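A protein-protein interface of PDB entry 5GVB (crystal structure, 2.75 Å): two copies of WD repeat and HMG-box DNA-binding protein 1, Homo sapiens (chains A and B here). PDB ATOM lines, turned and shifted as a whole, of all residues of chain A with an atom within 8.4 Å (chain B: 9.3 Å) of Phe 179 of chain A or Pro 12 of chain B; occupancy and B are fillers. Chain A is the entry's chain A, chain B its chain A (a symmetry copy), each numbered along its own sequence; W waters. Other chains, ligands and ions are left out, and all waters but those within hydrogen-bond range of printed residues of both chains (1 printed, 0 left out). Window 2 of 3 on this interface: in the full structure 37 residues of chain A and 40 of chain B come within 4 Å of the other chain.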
ATOM      1  N   PRO A  10      23.511 -24.021 -10.927  1.00  0.00           N
ATOM      2  CA  PRO A  10      24.182 -22.802 -11.389  1.00  0.00           C
ATOM      3  C   PRO A  10      25.560 -22.675 -10.748  1.00  0.00           C
ATOM      4  O   PRO A  10      25.719 -23.137  -9.616  1.00  0.00           O
ATOM      5  CB  PRO A  10      23.254 -21.695 -10.901  1.00  0.00           C
ATOM      6  CG  PRO A  10      22.698 -22.251  -9.625  1.00  0.00           C
ATOM      7  CD  PRO A  10      22.555 -23.741  -9.841  1.00  0.00           C
ATOM      8  N   MET A  11      26.539 -22.081 -11.430  1.00  0.00           N
ATOM      9  CA  MET A  11      27.864 -21.928 -10.816  1.00  0.00           C
ATOM     10  C   MET A  11      28.617 -20.624 -11.134  1.00  0.00           C
ATOM     11  O   MET A  11      28.499 -20.076 -12.235  1.00  0.00           O
ATOM     12  CB  MET A  11      28.740 -23.141 -11.161  1.00  0.00           C
ATOM     13  CG  MET A  11      28.255 -24.420 -10.489  1.00  0.00           C
ATOM     14  SD  MET A  11      29.100 -26.063 -11.054  1.00  0.00           S
ATOM     15  CE  MET A  11      30.914 -25.372 -11.222  1.00  0.00           C
ATOM     16  N   PRO A  12      29.403 -20.160 -10.154  1.00  0.00           N
ATOM     17  CA  PRO A  12      29.912 -18.780 -10.179  1.00  0.00           C
ATOM     18  C   PRO A  12      30.701 -18.465 -11.439  1.00  0.00           C
ATOM     19  O   PRO A  12      31.566 -19.233 -11.866  1.00  0.00           O
ATOM     20  CB  PRO A  12      30.801 -18.710  -8.930  1.00  0.00           C
ATOM     21  CG  PRO A  12      30.274 -19.767  -8.031  1.00  0.00           C
ATOM     22  CD  PRO A  12      29.813 -20.870  -8.929  1.00  0.00           C
ATOM     23  N   THR A  13      30.402 -17.319 -12.022  1.00  0.00           N
ATOM     24  CA  THR A  13      31.085 -16.889 -13.229  1.00  0.00           C
ATOM     25  C   THR A  13      32.447 -16.307 -12.874  1.00  0.00           C
ATOM     26  O   THR A  13      32.542 -15.490 -11.949  1.00  0.00           O
ATOM     27  CB  THR A  13      30.249 -15.853 -13.971  1.00  0.00           C
ATOM     28  OG1 THR A  13      28.904 -16.331 -14.106  1.00  0.00           O
ATOM     29  CG2 THR A  13      30.824 -15.583 -15.355  1.00  0.00           C
ATOM     30  N   PRO A  14      33.515 -16.716 -13.558  1.00  0.00           N
ATOM     31  CA  PRO A  14      34.806 -16.039 -13.385  1.00  0.00           C
ATOM     32  C   PRO A  14      34.647 -14.549 -13.625  1.00  0.00           C
ATOM     33  O   PRO A  14      34.085 -14.123 -14.638  1.00  0.00           O
ATOM     34  CB  PRO A  14      35.706 -16.688 -14.442  1.00  0.00           C
ATOM     35  CG  PRO A  14      34.999 -17.901 -14.898  1.00  0.00           C
ATOM     36  CD  PRO A  14      33.546 -17.742 -14.614  1.00  0.00           C
ATOM     37  N   GLY A 176      28.958  -7.960  -7.382  1.00  0.00           N
ATOM     38  CA  GLY A 176      29.052  -9.243  -6.726  1.00  0.00           C
ATOM     39  C   GLY A 176      29.394 -10.326  -7.725  1.00  0.00           C
ATOM     40  O   GLY A 176      30.040 -10.054  -8.742  1.00  0.00           O
ATOM     41  N   THR A 177      28.954 -11.550  -7.461  1.00  0.00           N
ATOM     42  CA  THR A 177      29.301 -12.701  -8.282  1.00  0.00           C
ATOM     43  C   THR A 177      28.111 -13.094  -9.146  1.00  0.00           C
ATOM     44  O   THR A 177      27.019 -13.353  -8.628  1.00  0.00           O
ATOM     45  CB  THR A 177      29.736 -13.877  -7.406  1.00  0.00           C
ATOM     46  OG1 THR A 177      30.907 -13.512  -6.666  1.00  0.00           O
ATOM     47  CG2 THR A 177      30.042 -15.095  -8.260  1.00  0.00           C
ATOM     48  N   GLY A 178      28.323 -13.134 -10.461  1.00  0.00           N
ATOM     49  CA  GLY A 178      27.313 -13.646 -11.361  1.00  0.00           C
ATOM     50  C   GLY A 178      27.344 -15.159 -11.443  1.00  0.00           C
ATOM     51  O   GLY A 178      28.285 -15.819 -11.004  1.00  0.00           O
ATOM     52  N   PHE A 179      26.285 -15.718 -12.021  1.00  0.00           N
ATOM     53  CA  PHE A 179      26.130 -17.162 -12.117  1.00  0.00           C
ATOM     54  C   PHE A 179      25.736 -17.561 -13.530  1.00  0.00           C
ATOM     55  O   PHE A 179      24.979 -16.851 -14.200  1.00  0.00           O
ATOM     56  CB  PHE A 179      25.085 -17.675 -11.117  1.00  0.00           C
ATOM     57  CG  PHE A 179      25.639 -17.936  -9.745  1.00  0.00           C
ATOM     58  CD1 PHE A 179      25.835 -16.897  -8.850  1.00  0.00           C
ATOM     59  CD2 PHE A 179      25.961 -19.225  -9.348  1.00  0.00           C
ATOM     60  CE1 PHE A 179      26.345 -17.137  -7.587  1.00  0.00           C
ATOM     61  CE2 PHE A 179      26.470 -19.471  -8.086  1.00  0.00           C
ATOM     62  CZ  PHE A 179      26.663 -18.426  -7.204  1.00  0.00           C
ATOM     63  N   ASP A 180      26.266 -18.703 -13.972  1.00  0.00           N
ATOM     64  CA  ASP A 180      25.926 -19.304 -15.263  1.00  0.00           C
ATOM     65  C   ASP A 180      26.285 -18.376 -16.424  1.00  0.00           C
ATOM     66  O   ASP A 180      25.482 -18.125 -17.325  1.00  0.00           O
ATOM     67  CB  ASP A 180      24.447 -19.704 -15.308  1.00  0.00           C
ATOM     68  CG  ASP A 180      24.201 -20.931 -16.165  1.00  0.00           C
ATOM     69  OD1 ASP A 180      24.410 -22.055 -15.663  1.00  0.00           O
ATOM     70  OD2 ASP A 180      23.796 -20.772 -17.336  1.00  0.00           O
ATOM     71  N   GLY A 181      27.516 -17.862 -16.395  1.00  0.00           N
ATOM     72  CA  GLY A 181      28.050 -17.073 -17.482  1.00  0.00           C
ATOM     73  C   GLY A 181      27.853 -15.577 -17.370  1.00  0.00           C
ATOM     74  O   GLY A 181      28.480 -14.830 -18.132  1.00  0.00           O
ATOM     75  N   ASP A 182      27.012 -15.111 -16.451  1.00  0.00           N
ATOM     76  CA  ASP A 182      26.719 -13.691 -16.324  1.00  0.00           C
ATOM     77  C   ASP A 182      27.728 -13.002 -15.416  1.00  0.00           C
ATOM     78  O   ASP A 182      28.149 -13.559 -14.400  1.00  0.00           O
ATOM     79  CB  ASP A 182      25.311 -13.475 -15.765  1.00  0.00           C
ATOM     80  CG  ASP A 182      24.229 -13.955 -16.705  1.00  0.00           C
ATOM     81  OD1 ASP A 182      24.384 -13.772 -17.929  1.00  0.00           O
ATOM     82  OD2 ASP A 182      23.222 -14.510 -16.218  1.00  0.00           O
ATOM     83  N   GLN A 183      28.110 -11.785 -15.790  1.00  0.00           N
ATOM     84  CA  GLN A 183      28.817 -10.911 -14.872  1.00  0.00           C
ATOM     85  C   GLN A 183      27.811 -10.168 -13.993  1.00  0.00           C
ATOM     86  O   GLN A 183      26.601 -10.190 -14.231  1.00  0.00           O
ATOM     87  CB  GLN A 183      29.698  -9.920 -15.634  1.00  0.00           C
ATOM     88  CG  GLN A 183      30.760 -10.567 -16.513  1.00  0.00           C
ATOM     89  CD  GLN A 183      31.904 -11.163 -15.714  1.00  0.00           C
ATOM     90  OE1 GLN A 183      32.253 -10.669 -14.642  1.00  0.00           O
ATOM     91  NE2 GLN A 183      32.494 -12.233 -16.235  1.00  0.00           N
ATOM     92  N   CYS A 184      28.326  -9.505 -12.956  1.00  0.00           N
ATOM     93  CA  CYS A 184      27.504  -8.730 -12.023  1.00  0.00           C
ATOM     94  C   CYS A 184      28.212  -7.394 -11.800  1.00  0.00           C
ATOM     95  O   CYS A 184      28.902  -7.199 -10.797  1.00  0.00           O
ATOM     96  CB  CYS A 184      27.284  -9.498 -10.718  1.00  0.00           C
ATOM     97  SG  CYS A 184      25.875  -8.937  -9.735  1.00  0.00           S
ATOM     98  N   ARG A 209      22.997 -11.401 -21.506  1.00  0.00           N
ATOM     99  CA  ARG A 209      23.284 -12.583 -20.706  1.00  0.00           C
ATOM    100  C   ARG A 209      24.461 -13.359 -21.290  1.00  0.00           C
ATOM    101  O   ARG A 209      24.665 -13.405 -22.506  1.00  0.00           O
ATOM    102  CB  ARG A 209      22.049 -13.477 -20.624  1.00  0.00           C
ATOM    103  CG  ARG A 209      20.839 -12.780 -20.026  1.00  0.00           C
ATOM    104  CD  ARG A 209      20.762 -12.998 -18.525  1.00  0.00           C
ATOM    105  NE  ARG A 209      19.774 -14.014 -18.175  1.00  0.00           N
ATOM    106  CZ  ARG A 209      19.771 -14.697 -17.034  1.00  0.00           C
ATOM    107  NH1 ARG A 209      20.715 -14.479 -16.127  1.00  0.00           N
ATOM    108  NH2 ARG A 209      18.828 -15.599 -16.801  1.00  0.00           N
ATOM    109  N   LYS A 210      25.246 -13.964 -20.394  1.00  0.00           N
ATOM    110  CA  LYS A 210      26.431 -14.741 -20.761  1.00  0.00           C
ATOM    111  C   LYS A 210      27.434 -13.908 -21.554  1.00  0.00           C
ATOM    112  O   LYS A 210      28.135 -14.423 -22.429  1.00  0.00           O
ATOM    113  CB  LYS A 210      26.047 -16.006 -21.537  1.00  0.00           C
ATOM    114  CG  LYS A 210      25.233 -17.001 -20.723  1.00  0.00           C
ATOM    115  CD  LYS A 210      24.770 -18.169 -21.576  1.00  0.00           C
ATOM    116  CE  LYS A 210      24.014 -19.197 -20.747  1.00  0.00           C
ATOM    117  NZ  LYS A 210      24.876 -19.820 -19.705  1.00  0.00           N
ATOM    118  N   PRO B  10      25.997 -22.920   2.456  1.00  0.00           N
ATOM    119  CA  PRO B  10      24.884 -22.235   1.791  1.00  0.00           C
ATOM    120  C   PRO B  10      24.852 -22.583   0.307  1.00  0.00           C
ATOM    121  O   PRO B  10      25.922 -22.823  -0.257  1.00  0.00           O
ATOM    122  CB  PRO B  10      25.219 -20.761   1.994  1.00  0.00           C
ATOM    123  CG  PRO B  10      26.718 -20.744   1.970  1.00  0.00           C
ATOM    124  CD  PRO B  10      27.165 -22.036   2.617  1.00  0.00           C
ATOM    125  N   MET B  11      23.678 -22.626  -0.323  1.00  0.00           N
ATOM    126  CA  MET B  11      23.633 -22.934  -1.757  1.00  0.00           C
ATOM    127  C   MET B  11      22.577 -22.181  -2.585  1.00  0.00           C
ATOM    128  O   MET B  11      21.485 -21.878  -2.094  1.00  0.00           O
ATOM    129  CB  MET B  11      23.479 -24.450  -1.960  1.00  0.00           C
ATOM    130  CG  MET B  11      24.722 -25.223  -1.534  1.00  0.00           C
ATOM    131  SD  MET B  11      24.560 -27.147  -1.479  1.00  0.00           S
ATOM    132  CE  MET B  11      23.464 -27.358  -3.077  1.00  0.00           C
ATOM    133  N   PRO B  12      22.925 -21.907  -3.850  1.00  0.00           N
ATOM    134  CA  PRO B  12      22.179 -20.920  -4.645  1.00  0.00           C
ATOM    135  C   PRO B  12      20.698 -21.247  -4.752  1.00  0.00           C
ATOM    136  O   PRO B  12      20.307 -22.383  -5.030  1.00  0.00           O
ATOM    137  CB  PRO B  12      22.865 -20.982  -6.016  1.00  0.00           C
ATOM    138  CG  PRO B  12      24.229 -21.496  -5.734  1.00  0.00           C
ATOM    139  CD  PRO B  12      24.074 -22.453  -4.596  1.00  0.00           C
ATOM    140  N   THR B  13      19.879 -20.233  -4.541  1.00  0.00           N
ATOM    141  CA  THR B  13      18.439 -20.402  -4.620  1.00  0.00           C
ATOM    142  C   THR B  13      17.997 -20.404  -6.077  1.00  0.00           C
ATOM    143  O   THR B  13      18.424 -19.534  -6.848  1.00  0.00           O
ATOM    144  CB  THR B  13      17.732 -19.286  -3.858  1.00  0.00           C
ATOM    145  OG1 THR B  13      18.313 -19.155  -2.554  1.00  0.00           O
ATOM    146  CG2 THR B  13      16.247 -19.585  -3.716  1.00  0.00           C
ATOM    147  N   PRO B  14      17.174 -21.365  -6.494  1.00  0.00           N
ATOM    148  CA  PRO B  14      16.570 -21.291  -7.830  1.00  0.00           C
ATOM    149  C   PRO B  14      15.853 -19.964  -8.002  1.00  0.00           C
ATOM    150  O   PRO B  14      15.051 -19.559  -7.158  1.00  0.00           O
ATOM    151  CB  PRO B  14      15.590 -22.469  -7.856  1.00  0.00           C
ATOM    152  CG  PRO B  14      15.942 -23.324  -6.706  1.00  0.00           C
ATOM    153  CD  PRO B  14      16.671 -22.499  -5.702  1.00  0.00           C
ATOM    154  N   ARG B  15      16.164 -19.274  -9.091  1.00  0.00           N
ATOM    155  CA  ARG B  15      15.654 -17.924  -9.269  1.00  0.00           C
ATOM    156  C   ARG B  15      14.257 -17.966  -9.868  1.00  0.00           C
ATOM    157  O   ARG B  15      14.044 -18.506 -10.960  1.00  0.00           O
ATOM    158  CB  ARG B  15      16.613 -17.087 -10.107  1.00  0.00           C
ATOM    159  CG  ARG B  15      18.051 -17.333  -9.713  1.00  0.00           C
ATOM    160  CD  ARG B  15      18.883 -16.084  -9.847  1.00  0.00           C
ATOM    161  NE  ARG B  15      18.781 -15.532 -11.188  1.00  0.00           N
ATOM    162  CZ  ARG B  15      19.627 -14.635 -11.672  1.00  0.00           C
ATOM    163  NH1 ARG B  15      20.646 -14.209 -10.924  1.00  0.00           N
ATOM    164  NH2 ARG B  15      19.471 -14.171 -12.902  1.00  0.00           N
ATOM    165  N   PRO B 158      16.978 -10.281 -15.284  1.00  0.00           N
ATOM    166  CA  PRO B 158      15.747 -10.930 -15.757  1.00  0.00           C
ATOM    167  C   PRO B 158      14.539 -10.481 -14.949  1.00  0.00           C
ATOM    168  O   PRO B 158      14.574 -10.435 -13.717  1.00  0.00           O
ATOM    169  CB  PRO B 158      16.036 -12.423 -15.563  1.00  0.00           C
ATOM    170  CG  PRO B 158      17.525 -12.523 -15.539  1.00  0.00           C
ATOM    171  CD  PRO B 158      18.006 -11.259 -14.894  1.00  0.00           C
ATOM    172  N   ARG B 175      18.448  -8.881  -8.889  1.00  0.00           N
ATOM    173  CA  ARG B 175      19.748  -8.236  -8.702  1.00  0.00           C
ATOM    174  C   ARG B 175      20.880  -9.232  -8.884  1.00  0.00           C
ATOM    175  O   ARG B 175      21.907  -8.917  -9.498  1.00  0.00           O
ATOM    176  CB  ARG B 175      19.861  -7.616  -7.311  1.00  0.00           C
ATOM    177  CG  ARG B 175      18.809  -6.617  -6.935  1.00  0.00           C
ATOM    178  CD  ARG B 175      18.564  -6.681  -5.438  1.00  0.00           C
ATOM    179  NE  ARG B 175      19.803  -6.667  -4.668  1.00  0.00           N
ATOM    180  CZ  ARG B 175      19.903  -7.091  -3.413  1.00  0.00           C
ATOM    181  NH1 ARG B 175      18.836  -7.573  -2.788  1.00  0.00           N
ATOM    182  NH2 ARG B 175      21.069  -7.043  -2.784  1.00  0.00           N
ATOM    183  N   GLY B 176      20.720 -10.427  -8.326  1.00  0.00           N
ATOM    184  CA  GLY B 176      21.731 -11.457  -8.367  1.00  0.00           C
ATOM    185  C   GLY B 176      21.179 -12.763  -7.842  1.00  0.00           C
ATOM    186  O   GLY B 176      19.974 -13.015  -7.940  1.00  0.00           O
ATOM    187  N   THR B 177      22.040 -13.593  -7.265  1.00  0.00           N
ATOM    188  CA  THR B 177      21.662 -14.924  -6.814  1.00  0.00           C
ATOM    189  C   THR B 177      21.537 -14.937  -5.297  1.00  0.00           C
ATOM    190  O   THR B 177      22.487 -14.586  -4.588  1.00  0.00           O
ATOM    191  CB  THR B 177      22.687 -15.961  -7.274  1.00  0.00           C
ATOM    192  OG1 THR B 177      22.725 -15.991  -8.706  1.00  0.00           O
ATOM    193  CG2 THR B 177      22.322 -17.341  -6.753  1.00  0.00           C
ATOM    194  N   GLY B 178      20.366 -15.337  -4.803  1.00  0.00           N
ATOM    195  CA  GLY B 178      20.190 -15.539  -3.382  1.00  0.00           C
ATOM    196  C   GLY B 178      20.693 -16.899  -2.938  1.00  0.00           C
ATOM    197  O   GLY B 178      20.959 -17.792  -3.740  1.00  0.00           O
ATOM    198  N   PHE B 179      20.824 -17.053  -1.623  1.00  0.00           N
ATOM    199  CA  PHE B 179      21.358 -18.274  -1.039  1.00  0.00           C
ATOM    200  C   PHE B 179      20.473 -18.750   0.102  1.00  0.00           C
ATOM    201  O   PHE B 179      19.922 -17.940   0.855  1.00  0.00           O
ATOM    202  CB  PHE B 179      22.793 -18.066  -0.537  1.00  0.00           C
ATOM    203  CG  PHE B 179      23.839 -18.248  -1.601  1.00  0.00           C
ATOM    204  CD1 PHE B 179      24.115 -17.233  -2.503  1.00  0.00           C
ATOM    205  CD2 PHE B 179      24.547 -19.436  -1.697  1.00  0.00           C
ATOM    206  CE1 PHE B 179      25.077 -17.400  -3.483  1.00  0.00           C
ATOM    207  CE2 PHE B 179      25.511 -19.608  -2.675  1.00  0.00           C
ATOM    208  CZ  PHE B 179      25.776 -18.590  -3.569  1.00  0.00           C
ATOM    209  N   ASP B 180      20.341 -20.073   0.212  1.00  0.00           N
ATOM    210  CA  ASP B 180      19.616 -20.723   1.305  1.00  0.00           C
ATOM    211  C   ASP B 180      18.144 -20.305   1.327  1.00  0.00           C
ATOM    212  O   ASP B 180      17.594 -19.927   2.363  1.00  0.00           O
ATOM    213  CB  ASP B 180      20.292 -20.447   2.652  1.00  0.00           C
ATOM    214  CG  ASP B 180      20.137 -21.596   3.628  1.00  0.00           C
ATOM    215  OD1 ASP B 180      20.914 -22.569   3.525  1.00  0.00           O
ATOM    216  OD2 ASP B 180      19.245 -21.526   4.500  1.00  0.00           O
ATOM    217  N   GLY B 181      17.505 -20.378   0.159  1.00  0.00           N
ATOM    218  CA  GLY B 181      16.083 -20.142   0.040  1.00  0.00           C
ATOM    219  C   GLY B 181      15.675 -18.720  -0.279  1.00  0.00           C
ATOM    220  O   GLY B 181      14.508 -18.493  -0.623  1.00  0.00           O
ATOM    221  N   ASP B 182      16.587 -17.757  -0.181  1.00  0.00           N
ATOM    222  CA  ASP B 182      16.258 -16.357  -0.406  1.00  0.00           C
ATOM    223  C   ASP B 182      16.373 -15.998  -1.881  1.00  0.00           C
ATOM    224  O   ASP B 182      17.283 -16.456  -2.575  1.00  0.00           O
ATOM    225  CB  ASP B 182      17.178 -15.445   0.406  1.00  0.00           C
ATOM    226  CG  ASP B 182      16.983 -15.596   1.898  1.00  0.00           C
ATOM    227  OD1 ASP B 182      15.823 -15.757   2.330  1.00  0.00           O
ATOM    228  OD2 ASP B 182      17.988 -15.547   2.637  1.00  0.00           O
ATOM    229  N   GLN B 183      15.444 -15.172  -2.352  1.00  0.00           N
ATOM    230  CA  GLN B 183      15.611 -14.518  -3.637  1.00  0.00           C
ATOM    231  C   GLN B 183      16.446 -13.249  -3.463  1.00  0.00           C
ATOM    232  O   GLN B 183      16.713 -12.797  -2.347  1.00  0.00           O
ATOM    233  CB  GLN B 183      14.254 -14.187  -4.259  1.00  0.00           C
ATOM    234  CG  GLN B 183      13.362 -15.395  -4.507  1.00  0.00           C
ATOM    235  CD  GLN B 183      13.830 -16.245  -5.674  1.00  0.00           C
ATOM    236  OE1 GLN B 183      14.409 -15.738  -6.634  1.00  0.00           O
ATOM    237  NE2 GLN B 183      13.581 -17.547  -5.593  1.00  0.00           N
HETATM  238  O   HOH W   1      23.372 -14.745 -12.699  1.00  0.00           O
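The guanidinium group (NH2) of Arg 15 of chain B lies close to the guanidinium group (NH1) of Arg 209 of chain A (3.5 Å).
N of Phe 179 of chain A lies within hydrogen-bond range of OG1 of Thr 13 of chain A, at 3.4 Å.
The backbone carbonyl oxygen of Cys 184 of chain A is in hydrogen-bond range of the backbone NH of Gly 176 of chain A (3.5 Å).
The side-chain carboxylate of Asp 182 of chain A lies within salt-bridge range of the guanidinium group of Arg 209 of chain A.
The side-chain hydroxyl of Thr 13 of chain B is in hydrogen-bond range of the backbone NH of Phe 179 of chain B, at 3.4 Å.
The guanidinium group (NH1) of Arg 15 of chain B lies within hydrogen-bond range of the backbone carbonyl oxygen (O) of Gly 176 of chain B, at 3.3 Å.
CG of Pro 10 of chain A touches CB of Pro 12 of chain B (3.8 Å).
Pro 12 of chain B touches Phe 179 of chain A.
OG1 of Thr 177 of chain B touches CD1 of Phe 179 of chain A (3.2 Å).
Phe 179 of chain A touches Phe 179 of chain B.
Arg 175 of chain B touches Cys 184 of chain A (O to SG, 3.98 Å).
CZ of Arg 209 of chain A touches CG of Pro 158 of chain B (3.5 Å).
Phe 179 of chain A touches just these residues of chain B: Pro 12, Thr 177 and Phe 179.
Pro 12 of chain B touches two residues of chain A.
No residue of chain B comes within 4 Å of Asp 180 of chain A.
No residue of chain B comes within 4 Å of Asp 182 of chain A.
Of the printed residues of chain B, Cys 184 of chain A touches Arg 175.
Of the printed residues of chain A, Phe 179 of chain B touches Phe 179.
Of the printed residues of chain A, Arg 15 of chain B touches Arg 209.
Of the printed residues of chain B, Arg 209 of chain A touches Arg 15 and Pro 158.
Printed residues of chain A within 4 Å of Arg 175 of chain B: Cys 184 (3.98 Å).
The nearest residue of chain B that does not touch Phe 179 of chain A is Arg 15 of chain B (5.6 Å).
The nearest residue of chain A that does not touch Pro 12 of chain B is Met 11 of chain A (6.2 Å).
Hydrophobic or aromatic side chains of chain A within 4 Å of the printed part of chain B: Pro 10 and Phe 179.
Among the printed residues, 7 pairs touch across the chains.
Pro 10 of chain A touches Pro 12 of chain B, but with the chains exchanged Pro 12 of chain A does not touch Pro 10 of chain B (9.4 Å).
Phe 179 of chain A touches Pro 12 of chain B, but with the chains exchanged Pro 12 of chain A does not touch Phe 179 of chain B (6.4 Å).
Phe 179 of chain A touches Thr 177 of chain B, but with the chains exchanged Thr 177 of chain A does not touch Phe 179 of chain B (6.8 Å).
Phe 179 of chain A touches its own counterpart, Phe 179 of chain B.
13 positions are printed for both chains.
Of the 7 pairs that touch across the chains among the printed residues, 1 has its exchanged pair printed and touching as well.
Water W1 bridges O of Phe 179 of chain A (3.0 Å) and NH1 of Arg 15 of chain B (3.3 Å).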
